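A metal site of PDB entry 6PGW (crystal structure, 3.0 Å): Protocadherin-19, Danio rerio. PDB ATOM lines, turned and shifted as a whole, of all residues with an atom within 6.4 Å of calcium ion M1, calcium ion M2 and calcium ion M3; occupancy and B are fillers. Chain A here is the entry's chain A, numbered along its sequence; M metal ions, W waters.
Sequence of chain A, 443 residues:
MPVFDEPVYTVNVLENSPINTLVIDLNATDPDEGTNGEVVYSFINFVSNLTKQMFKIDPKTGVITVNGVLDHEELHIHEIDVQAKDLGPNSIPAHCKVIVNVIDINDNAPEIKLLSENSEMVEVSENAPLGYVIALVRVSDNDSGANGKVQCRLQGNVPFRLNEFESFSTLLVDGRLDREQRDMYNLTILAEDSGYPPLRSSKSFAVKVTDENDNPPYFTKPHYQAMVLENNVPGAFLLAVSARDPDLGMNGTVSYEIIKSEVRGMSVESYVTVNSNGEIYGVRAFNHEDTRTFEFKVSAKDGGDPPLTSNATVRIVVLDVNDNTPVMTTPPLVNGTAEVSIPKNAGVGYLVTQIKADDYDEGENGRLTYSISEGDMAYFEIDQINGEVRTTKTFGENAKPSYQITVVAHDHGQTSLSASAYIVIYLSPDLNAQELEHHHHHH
ND2 of Asn 108 sits close to OD1 of Asp 107. The side-chain carboxylate (OD1) of Asp 193 sits close to the backbone NH (N) of Gly 195 (3.4 Å). OE2 of Glu 73 lies close to ND2 of Asn 108. The backbone NH (N) of His 72 sits close to the side-chain carboxylate (OE2) of Glu 15 (2.9 Å). The side-chain amide nitrogen (ND2) of Asn 16 lies close to the side-chain carboxylate (OD2) of Asp 107. OD1 of Asp 193 lies within hydrogen-bond range of N of Leu 199 (2.5 Å). O of Ile 103 sits at hydrogen-bond distance from N of Glu 15, at 3.2 Å. N of Ser 144 lies within hydrogen-bond range of OD2 of Asp 104 (3.0 Å).
Of the 28 residues printed, 4 come within 4 Å of calcium ion M1. Along chain A the residues within 4 Å of calcium ion M1 span positions 15 to 107.
Of the 28 residues printed, 7 come within 4 Å of calcium ion M2.
Of the 28 residues printed, 6 come within 4 Å of calcium ion M3.
Calcium ion M1 is bound by OE2 of Glu 15 (2.3 Å), OD1 of Asp 71 (2.3 Å), water W1 (2.3 Å), OE2 of Glu 73 (2.3 Å), water W2 (2.3 Å) and OD2 of Asp 107 (2.3 Å).
Calcium ion M2 is bound by the side-chain carboxylate of Asp 143, the side-chain carboxylate of Asp 104, the backbone carbonyl oxygen of Ile 105, the side-chain carboxylate of Glu 73, the side-chain carboxylate of Glu 15 and the side-chain carboxylate of Asp 107.
Calcium ion M3 is bound by O of Asn 108, OD1 of Asn 106, OD2 of Asp 141, O of Asn 147, OD2 of Asp 143, OD1 of Asp 141 and OD2 of Asp 193.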
ATOM      1  N   GLU A  15      19.325  18.320 -10.827  1.00  0.00           N
ATOM      2  CA  GLU A  15      18.910  18.333  -9.417  1.00  0.00           C
ATOM      3  C   GLU A  15      18.434  19.721  -8.946  1.00  0.00           C
ATOM      4  O   GLU A  15      18.997  20.724  -9.293  1.00  0.00           O
ATOM      5  CB  GLU A  15      20.101  17.835  -8.575  1.00  0.00           C
ATOM      6  CG  GLU A  15      20.054  18.100  -7.096  1.00  0.00           C
ATOM      7  CD  GLU A  15      20.993  17.169  -6.319  1.00  0.00           C
ATOM      8  OE1 GLU A  15      22.219  17.044  -6.616  1.00  0.00           O
ATOM      9  OE2 GLU A  15      20.500  16.535  -5.388  1.00  0.00           O
ATOM     10  N   ASN A  16      17.370  19.750  -8.187  1.00  0.00           N
ATOM     11  CA  ASN A  16      16.795  20.991  -7.675  1.00  0.00           C
ATOM     12  C   ASN A  16      16.378  22.016  -8.733  1.00  0.00           C
ATOM     13  O   ASN A  16      16.278  23.174  -8.442  1.00  0.00           O
ATOM     14  CB  ASN A  16      17.736  21.624  -6.627  1.00  0.00           C
ATOM     15  CG  ASN A  16      18.200  20.632  -5.585  1.00  0.00           C
ATOM     16  OD1 ASN A  16      17.480  19.672  -5.242  1.00  0.00           O
ATOM     17  ND2 ASN A  16      19.388  20.837  -5.061  1.00  0.00           N
ATOM     18  N   LEU A  70      13.822  17.580  -7.325  1.00  0.00           N
ATOM     19  CA  LEU A  70      14.521  16.446  -7.812  1.00  0.00           C
ATOM     20  C   LEU A  70      15.785  16.301  -7.001  1.00  0.00           C
ATOM     21  O   LEU A  70      16.768  16.946  -7.290  1.00  0.00           O
ATOM     22  CB  LEU A  70      14.825  16.618  -9.314  1.00  0.00           C
ATOM     23  CG  LEU A  70      13.584  16.593 -10.223  1.00  0.00           C
ATOM     24  CD1 LEU A  70      13.883  17.187 -11.584  1.00  0.00           C
ATOM     25  CD2 LEU A  70      13.047  15.168 -10.363  1.00  0.00           C
ATOM     26  N   ASP A  71      15.749  15.456  -5.974  1.00  0.00           N
ATOM     27  CA  ASP A  71      16.926  15.203  -5.117  1.00  0.00           C
ATOM     28  C   ASP A  71      17.783  13.967  -5.535  1.00  0.00           C
ATOM     29  O   ASP A  71      17.460  12.847  -5.207  1.00  0.00           O
ATOM     30  CB  ASP A  71      16.460  15.057  -3.664  1.00  0.00           C
ATOM     31  CG  ASP A  71      17.612  14.997  -2.673  1.00  0.00           C
ATOM     32  OD1 ASP A  71      18.736  15.449  -3.018  1.00  0.00           O
ATOM     33  OD2 ASP A  71      17.409  14.504  -1.530  1.00  0.00           O
ATOM     34  N   HIS A  72      18.931  14.194  -6.194  1.00  0.00           N
ATOM     35  CA  HIS A  72      19.919  13.094  -6.471  1.00  0.00           C
ATOM     36  C   HIS A  72      20.235  12.140  -5.303  1.00  0.00           C
ATOM     37  O   HIS A  72      20.523  10.942  -5.529  1.00  0.00           O
ATOM     38  CB  HIS A  72      21.261  13.646  -7.010  1.00  0.00           C
ATOM     39  CG  HIS A  72      22.219  12.563  -7.451  1.00  0.00           C
ATOM     40  ND1 HIS A  72      22.175  11.990  -8.711  1.00  0.00           N
ATOM     41  CD2 HIS A  72      23.238  11.947  -6.798  1.00  0.00           C
ATOM     42  CE1 HIS A  72      23.124  11.072  -8.806  1.00  0.00           C
ATOM     43  NE2 HIS A  72      23.781  11.032  -7.665  1.00  0.00           N
ATOM     44  N   GLU A  73      20.248  12.659  -4.095  1.00  0.00           N
ATOM     45  CA  GLU A  73      20.555  11.841  -2.934  1.00  0.00           C
ATOM     46  C   GLU A  73      19.342  10.938  -2.584  1.00  0.00           C
ATOM     47  O   GLU A  73      19.502   9.889  -1.957  1.00  0.00           O
ATOM     48  CB  GLU A  73      20.987  12.735  -1.773  1.00  0.00           C
ATOM     49  CG  GLU A  73      22.366  13.382  -1.976  1.00  0.00           C
ATOM     50  CD  GLU A  73      22.387  14.546  -2.950  1.00  0.00           C
ATOM     51  OE1 GLU A  73      23.269  14.568  -3.842  1.00  0.00           O
ATOM     52  OE2 GLU A  73      21.535  15.485  -2.827  1.00  0.00           O
ATOM     53  N   GLU A  74      18.167  11.333  -3.035  1.00  0.00           N
ATOM     54  CA  GLU A  74      16.920  10.603  -2.800  1.00  0.00           C
ATOM     55  C   GLU A  74      16.721   9.645  -3.967  1.00  0.00           C
ATOM     56  O   GLU A  74      16.925   8.442  -3.821  1.00  0.00           O
ATOM     57  CB  GLU A  74      15.780  11.620  -2.695  1.00  0.00           C
ATOM     58  CG  GLU A  74      14.371  11.136  -2.400  1.00  0.00           C
ATOM     59  CD  GLU A  74      13.332  12.268  -2.614  1.00  0.00           C
ATOM     60  OE1 GLU A  74      13.413  12.980  -3.669  1.00  0.00           O
ATOM     61  OE2 GLU A  74      12.455  12.475  -1.722  1.00  0.00           O
ATOM     62  N   ILE A 103      20.873  14.734 -12.604  1.00  0.00           N
ATOM     63  CA  ILE A 103      22.268  15.021 -12.566  1.00  0.00           C
ATOM     64  C   ILE A 103      22.597  15.624 -11.222  1.00  0.00           C
ATOM     65  O   ILE A 103      21.973  16.597 -10.809  1.00  0.00           O
ATOM     66  CB  ILE A 103      22.669  15.980 -13.697  1.00  0.00           C
ATOM     67  CG1 ILE A 103      22.873  15.210 -15.042  1.00  0.00           C
ATOM     68  CG2 ILE A 103      23.974  16.669 -13.363  1.00  0.00           C
ATOM     69  CD1 ILE A 103      21.801  14.176 -15.435  1.00  0.00           C
ATOM     70  N   ASP A 104      23.558  14.997 -10.539  1.00  0.00           N
ATOM     71  CA  ASP A 104      24.060  15.420  -9.206  1.00  0.00           C
ATOM     72  C   ASP A 104      24.736  16.757  -9.280  1.00  0.00           C
ATOM     73  O   ASP A 104      25.577  16.971 -10.124  1.00  0.00           O
ATOM     74  CB  ASP A 104      25.091  14.428  -8.691  1.00  0.00           C
ATOM     75  CG  ASP A 104      25.614  14.794  -7.339  1.00  0.00           C
ATOM     76  OD1 ASP A 104      24.835  15.335  -6.516  1.00  0.00           O
ATOM     77  OD2 ASP A 104      26.802  14.520  -7.084  1.00  0.00           O
ATOM     78  N   ILE A 105      24.377  17.653  -8.356  1.00  0.00           N
ATOM     79  CA  ILE A 105      25.106  18.919  -8.161  1.00  0.00           C
ATOM     80  C   ILE A 105      25.568  19.048  -6.693  1.00  0.00           C
ATOM     81  O   ILE A 105      25.167  18.229  -5.829  1.00  0.00           O
ATOM     82  CB  ILE A 105      24.267  20.136  -8.658  1.00  0.00           C
ATOM     83  CG1 ILE A 105      23.067  20.387  -7.767  1.00  0.00           C
ATOM     84  CG2 ILE A 105      23.784  19.911 -10.088  1.00  0.00           C
ATOM     85  CD1 ILE A 105      22.135  21.421  -8.316  1.00  0.00           C
ATOM     86  N   ASN A 106      26.443  20.031  -6.425  1.00  0.00           N
ATOM     87  CA  ASN A 106      27.185  20.156  -5.181  1.00  0.00           C
ATOM     88  C   ASN A 106      26.368  20.991  -4.166  1.00  0.00           C
ATOM     89  O   ASN A 106      26.703  22.130  -3.827  1.00  0.00           O
ATOM     90  CB  ASN A 106      28.565  20.780  -5.462  1.00  0.00           C
ATOM     91  CG  ASN A 106      29.549  20.576  -4.329  1.00  0.00           C
ATOM     92  OD1 ASN A 106      29.377  19.672  -3.526  1.00  0.00           O
ATOM     93  ND2 ASN A 106      30.605  21.416  -4.268  1.00  0.00           N
ATOM     94  N   ASP A 107      25.275  20.393  -3.693  1.00  0.00           N
ATOM     95  CA  ASP A 107      24.326  21.073  -2.791  1.00  0.00           C
ATOM     96  C   ASP A 107      24.438  20.623  -1.303  1.00  0.00           C
ATOM     97  O   ASP A 107      23.873  21.255  -0.445  1.00  0.00           O
ATOM     98  CB  ASP A 107      22.862  20.982  -3.336  1.00  0.00           C
ATOM     99  CG  ASP A 107      22.343  19.537  -3.502  1.00  0.00           C
ATOM    100  OD1 ASP A 107      23.157  18.553  -3.680  1.00  0.00           O
ATOM    101  OD2 ASP A 107      21.083  19.387  -3.495  1.00  0.00           O
ATOM    102  N   ASN A 108      25.224  19.570  -1.035  1.00  0.00           N
ATOM    103  CA  ASN A 108      25.600  19.132   0.321  1.00  0.00           C
ATOM    104  C   ASN A 108      27.099  19.364   0.553  1.00  0.00           C
ATOM    105  O   ASN A 108      27.951  18.762  -0.103  1.00  0.00           O
ATOM    106  CB  ASN A 108      25.301  17.626   0.492  1.00  0.00           C
ATOM    107  CG  ASN A 108      23.843  17.271   0.313  1.00  0.00           C
ATOM    108  OD1 ASN A 108      23.103  17.237   1.264  1.00  0.00           O
ATOM    109  ND2 ASN A 108      23.456  16.936  -0.912  1.00  0.00           N
ATOM    110  N   ALA A 109      27.430  20.187   1.535  1.00  0.00           N
ATOM    111  CA  ALA A 109      28.824  20.409   1.919  1.00  0.00           C
ATOM    112  C   ALA A 109      29.216  19.408   2.992  1.00  0.00           C
ATOM    113  O   ALA A 109      28.386  18.656   3.437  1.00  0.00           O
ATOM    114  CB  ALA A 109      28.985  21.840   2.418  1.00  0.00           C
ATOM    115  N   PRO A 110      30.501  19.376   3.393  1.00  0.00           N
ATOM    116  CA  PRO A 110      30.906  18.340   4.318  1.00  0.00           C
ATOM    117  C   PRO A 110      30.249  18.409   5.726  1.00  0.00           C
ATOM    118  O   PRO A 110      29.744  19.460   6.165  1.00  0.00           O
ATOM    119  CB  PRO A 110      32.419  18.543   4.420  1.00  0.00           C
ATOM    120  CG  PRO A 110      32.793  19.107   3.108  1.00  0.00           C
ATOM    121  CD  PRO A 110      31.671  20.034   2.785  1.00  0.00           C
ATOM    122  N   ASP A 141      30.163  13.812   2.917  1.00  0.00           N
ATOM    123  CA  ASP A 141      29.447  14.682   1.962  1.00  0.00           C
ATOM    124  C   ASP A 141      28.478  13.755   1.273  1.00  0.00           C
ATOM    125  O   ASP A 141      28.846  12.639   0.892  1.00  0.00           O
ATOM    126  CB  ASP A 141      30.417  15.310   0.931  1.00  0.00           C
ATOM    127  CG  ASP A 141      29.789  16.461   0.142  1.00  0.00           C
ATOM    128  OD1 ASP A 141      28.762  16.255  -0.544  1.00  0.00           O
ATOM    129  OD2 ASP A 141      30.352  17.549   0.192  1.00  0.00           O
ATOM    130  N   ASN A 142      27.233  14.159   1.157  1.00  0.00           N
ATOM    131  CA  ASN A 142      26.181  13.252   0.746  1.00  0.00           C
ATOM    132  C   ASN A 142      26.027  13.233  -0.745  1.00  0.00           C
ATOM    133  O   ASN A 142      25.228  12.458  -1.258  1.00  0.00           O
ATOM    134  CB  ASN A 142      24.871  13.616   1.432  1.00  0.00           C
ATOM    135  CG  ASN A 142      24.911  13.349   2.932  1.00  0.00           C
ATOM    136  OD1 ASN A 142      25.961  13.480   3.570  1.00  0.00           O
ATOM    137  ND2 ASN A 142      23.793  12.956   3.490  1.00  0.00           N
ATOM    138  N   ASP A 143      26.790  14.055  -1.468  1.00  0.00           N
ATOM    139  CA  ASP A 143      26.776  14.008  -2.938  1.00  0.00           C
ATOM    140  C   ASP A 143      27.622  12.852  -3.450  1.00  0.00           C
ATOM    141  O   ASP A 143      28.284  12.130  -2.686  1.00  0.00           O
ATOM    142  CB  ASP A 143      27.285  15.319  -3.556  1.00  0.00           C
ATOM    143  CG  ASP A 143      26.550  16.547  -3.059  1.00  0.00           C
ATOM    144  OD1 ASP A 143      25.300  16.577  -3.174  1.00  0.00           O
ATOM    145  OD2 ASP A 143      27.245  17.491  -2.580  1.00  0.00           O
ATOM    146  N   SER A 144      27.605  12.715  -4.779  1.00  0.00           N
ATOM    147  CA  SER A 144      28.425  11.759  -5.514  1.00  0.00           C
ATOM    148  C   SER A 144      29.579  12.422  -6.230  1.00  0.00           C
ATOM    149  O   SER A 144      29.549  13.610  -6.491  1.00  0.00           O
ATOM    150  CB  SER A 144      27.543  11.041  -6.523  1.00  0.00           C
ATOM    151  OG  SER A 144      26.322  10.661  -5.908  1.00  0.00           O
ATOM    152  N   ALA A 146      33.333  13.857  -7.357  1.00  0.00           N
ATOM    153  CA  ALA A 146      34.126  14.967  -6.809  1.00  0.00           C
ATOM    154  C   ALA A 146      33.353  15.756  -5.758  1.00  0.00           C
ATOM    155  O   ALA A 146      33.923  16.203  -4.772  1.00  0.00           O
ATOM    156  CB  ALA A 146      34.538  15.898  -7.931  1.00  0.00           C
ATOM    157  N   ASN A 147      32.059  15.944  -6.015  1.00  0.00           N
ATOM    158  CA  ASN A 147      31.176  16.638  -5.112  1.00  0.00           C
ATOM    159  C   ASN A 147      31.017  15.886  -3.810  1.00  0.00           C
ATOM    160  O   ASN A 147      30.688  16.484  -2.777  1.00  0.00           O
ATOM    161  CB  ASN A 147      29.810  16.833  -5.751  1.00  0.00           C
ATOM    162  CG  ASN A 147      29.845  17.830  -6.878  1.00  0.00           C
ATOM    163  OD1 ASN A 147      30.807  18.553  -7.033  1.00  0.00           O
ATOM    164  ND2 ASN A 147      28.779  17.901  -7.633  1.00  0.00           N
ATOM    165  N   GLY A 148      31.258  14.575  -3.852  1.00  0.00           N
ATOM    166  CA  GLY A 148      31.300  13.754  -2.658  1.00  0.00           C
ATOM    167  C   GLY A 148      32.646  13.645  -1.942  1.00  0.00           C
ATOM    168  O   GLY A 148      32.657  13.387  -0.765  1.00  0.00           O
ATOM    169  N   LYS A 149      33.757  13.781  -2.672  1.00  0.00           N
ATOM    170  CA  LYS A 149      35.109  13.546  -2.081  1.00  0.00           C
ATOM    171  C   LYS A 149      35.566  14.639  -1.146  1.00  0.00           C
ATOM    172  O   LYS A 149      35.378  15.829  -1.417  1.00  0.00           O
ATOM    173  CB  LYS A 149      36.168  13.394  -3.180  1.00  0.00           C
ATOM    174  CG  LYS A 149      36.331  11.972  -3.676  1.00  0.00           C
ATOM    175  CD  LYS A 149      36.498  11.948  -5.202  1.00  0.00           C
ATOM    176  CE  LYS A 149      36.236  10.572  -5.810  1.00  0.00           C
ATOM    177  NZ  LYS A 149      36.063  10.660  -7.286  1.00  0.00           N
ATOM    178  N   VAL A 150      36.221  14.250  -0.056  1.00  0.00           N
ATOM    179  CA  VAL A 150      36.619  15.229   0.959  1.00  0.00           C
ATOM    180  C   VAL A 150      37.944  14.934   1.681  1.00  0.00           C
ATOM    181  O   VAL A 150      38.253  13.781   2.014  1.00  0.00           O
ATOM    182  CB  VAL A 150      35.508  15.377   2.009  1.00  0.00           C
ATOM    183  CG1 VAL A 150      34.140  15.562   1.342  1.00  0.00           C
ATOM    184  CG2 VAL A 150      35.464  14.160   2.920  1.00  0.00           C
ATOM    185  N   ASP A 193      34.843  19.875   0.374  1.00  0.00           N
ATOM    186  CA  ASP A 193      34.587  18.854  -0.679  1.00  0.00           C
ATOM    187  C   ASP A 193      35.374  19.154  -1.915  1.00  0.00           C
ATOM    188  O   ASP A 193      36.028  20.148  -1.976  1.00  0.00           O
ATOM    189  CB  ASP A 193      33.063  18.604  -0.945  1.00  0.00           C
ATOM    190  CG  ASP A 193      32.304  19.806  -1.571  1.00  0.00           C
ATOM    191  OD1 ASP A 193      32.925  20.713  -2.165  1.00  0.00           O
ATOM    192  OD2 ASP A 193      31.036  19.776  -1.491  1.00  0.00           O
ATOM    193  N   SER A 194      35.375  18.259  -2.885  1.00  0.00           N
ATOM    194  CA  SER A 194      36.189  18.448  -4.082  1.00  0.00           C
ATOM    195  C   SER A 194      35.403  18.886  -5.308  1.00  0.00           C
ATOM    196  O   SER A 194      35.855  18.698  -6.441  1.00  0.00           O
ATOM    197  CB  SER A 194      36.995  17.181  -4.378  1.00  0.00           C
ATOM    198  OG  SER A 194      37.547  16.656  -3.164  1.00  0.00           O
ATOM    199  N   GLY A 195      34.235  19.509  -5.085  1.00  0.00           N
ATOM    200  CA  GLY A 195      33.476  20.160  -6.168  1.00  0.00           C
ATOM    201  C   GLY A 195      34.148  21.443  -6.660  1.00  0.00           C
ATOM    202  O   GLY A 195      35.183  21.826  -6.147  1.00  0.00           O
ATOM    203  N   LEU A 199      33.135  23.193  -1.645  1.00  0.00           N
ATOM    204  CA  LEU A 199      32.388  23.705  -0.492  1.00  0.00           C
ATOM    205  C   LEU A 199      33.067  23.307   0.760  1.00  0.00           C
ATOM    206  O   LEU A 199      33.449  22.151   0.895  1.00  0.00           O
ATOM    207  CB  LEU A 199      30.963  23.167  -0.498  1.00  0.00           C
ATOM    208  CG  LEU A 199      30.016  24.045  -1.298  1.00  0.00           C
ATOM    209  CD1 LEU A 199      28.861  23.244  -1.869  1.00  0.00           C
ATOM    210  CD2 LEU A 199      29.496  25.166  -0.424  1.00  0.00           C
HETATM  211 CA    CA M   1      20.123  17.269  -3.288  1.00  0.00          CA
HETATM  212 CA    CA M   2      23.763  16.618  -4.887  1.00  0.00          CA
HETATM  213 CA    CA M   3      29.354  18.129  -1.809  1.00  0.00          CA
HETATM  214  O   HOH W   1      18.233  18.519  -2.792  1.00  0.00           O
HETATM  215  O   HOH W   2      19.821  17.030  -0.989  1.00  0.00           O
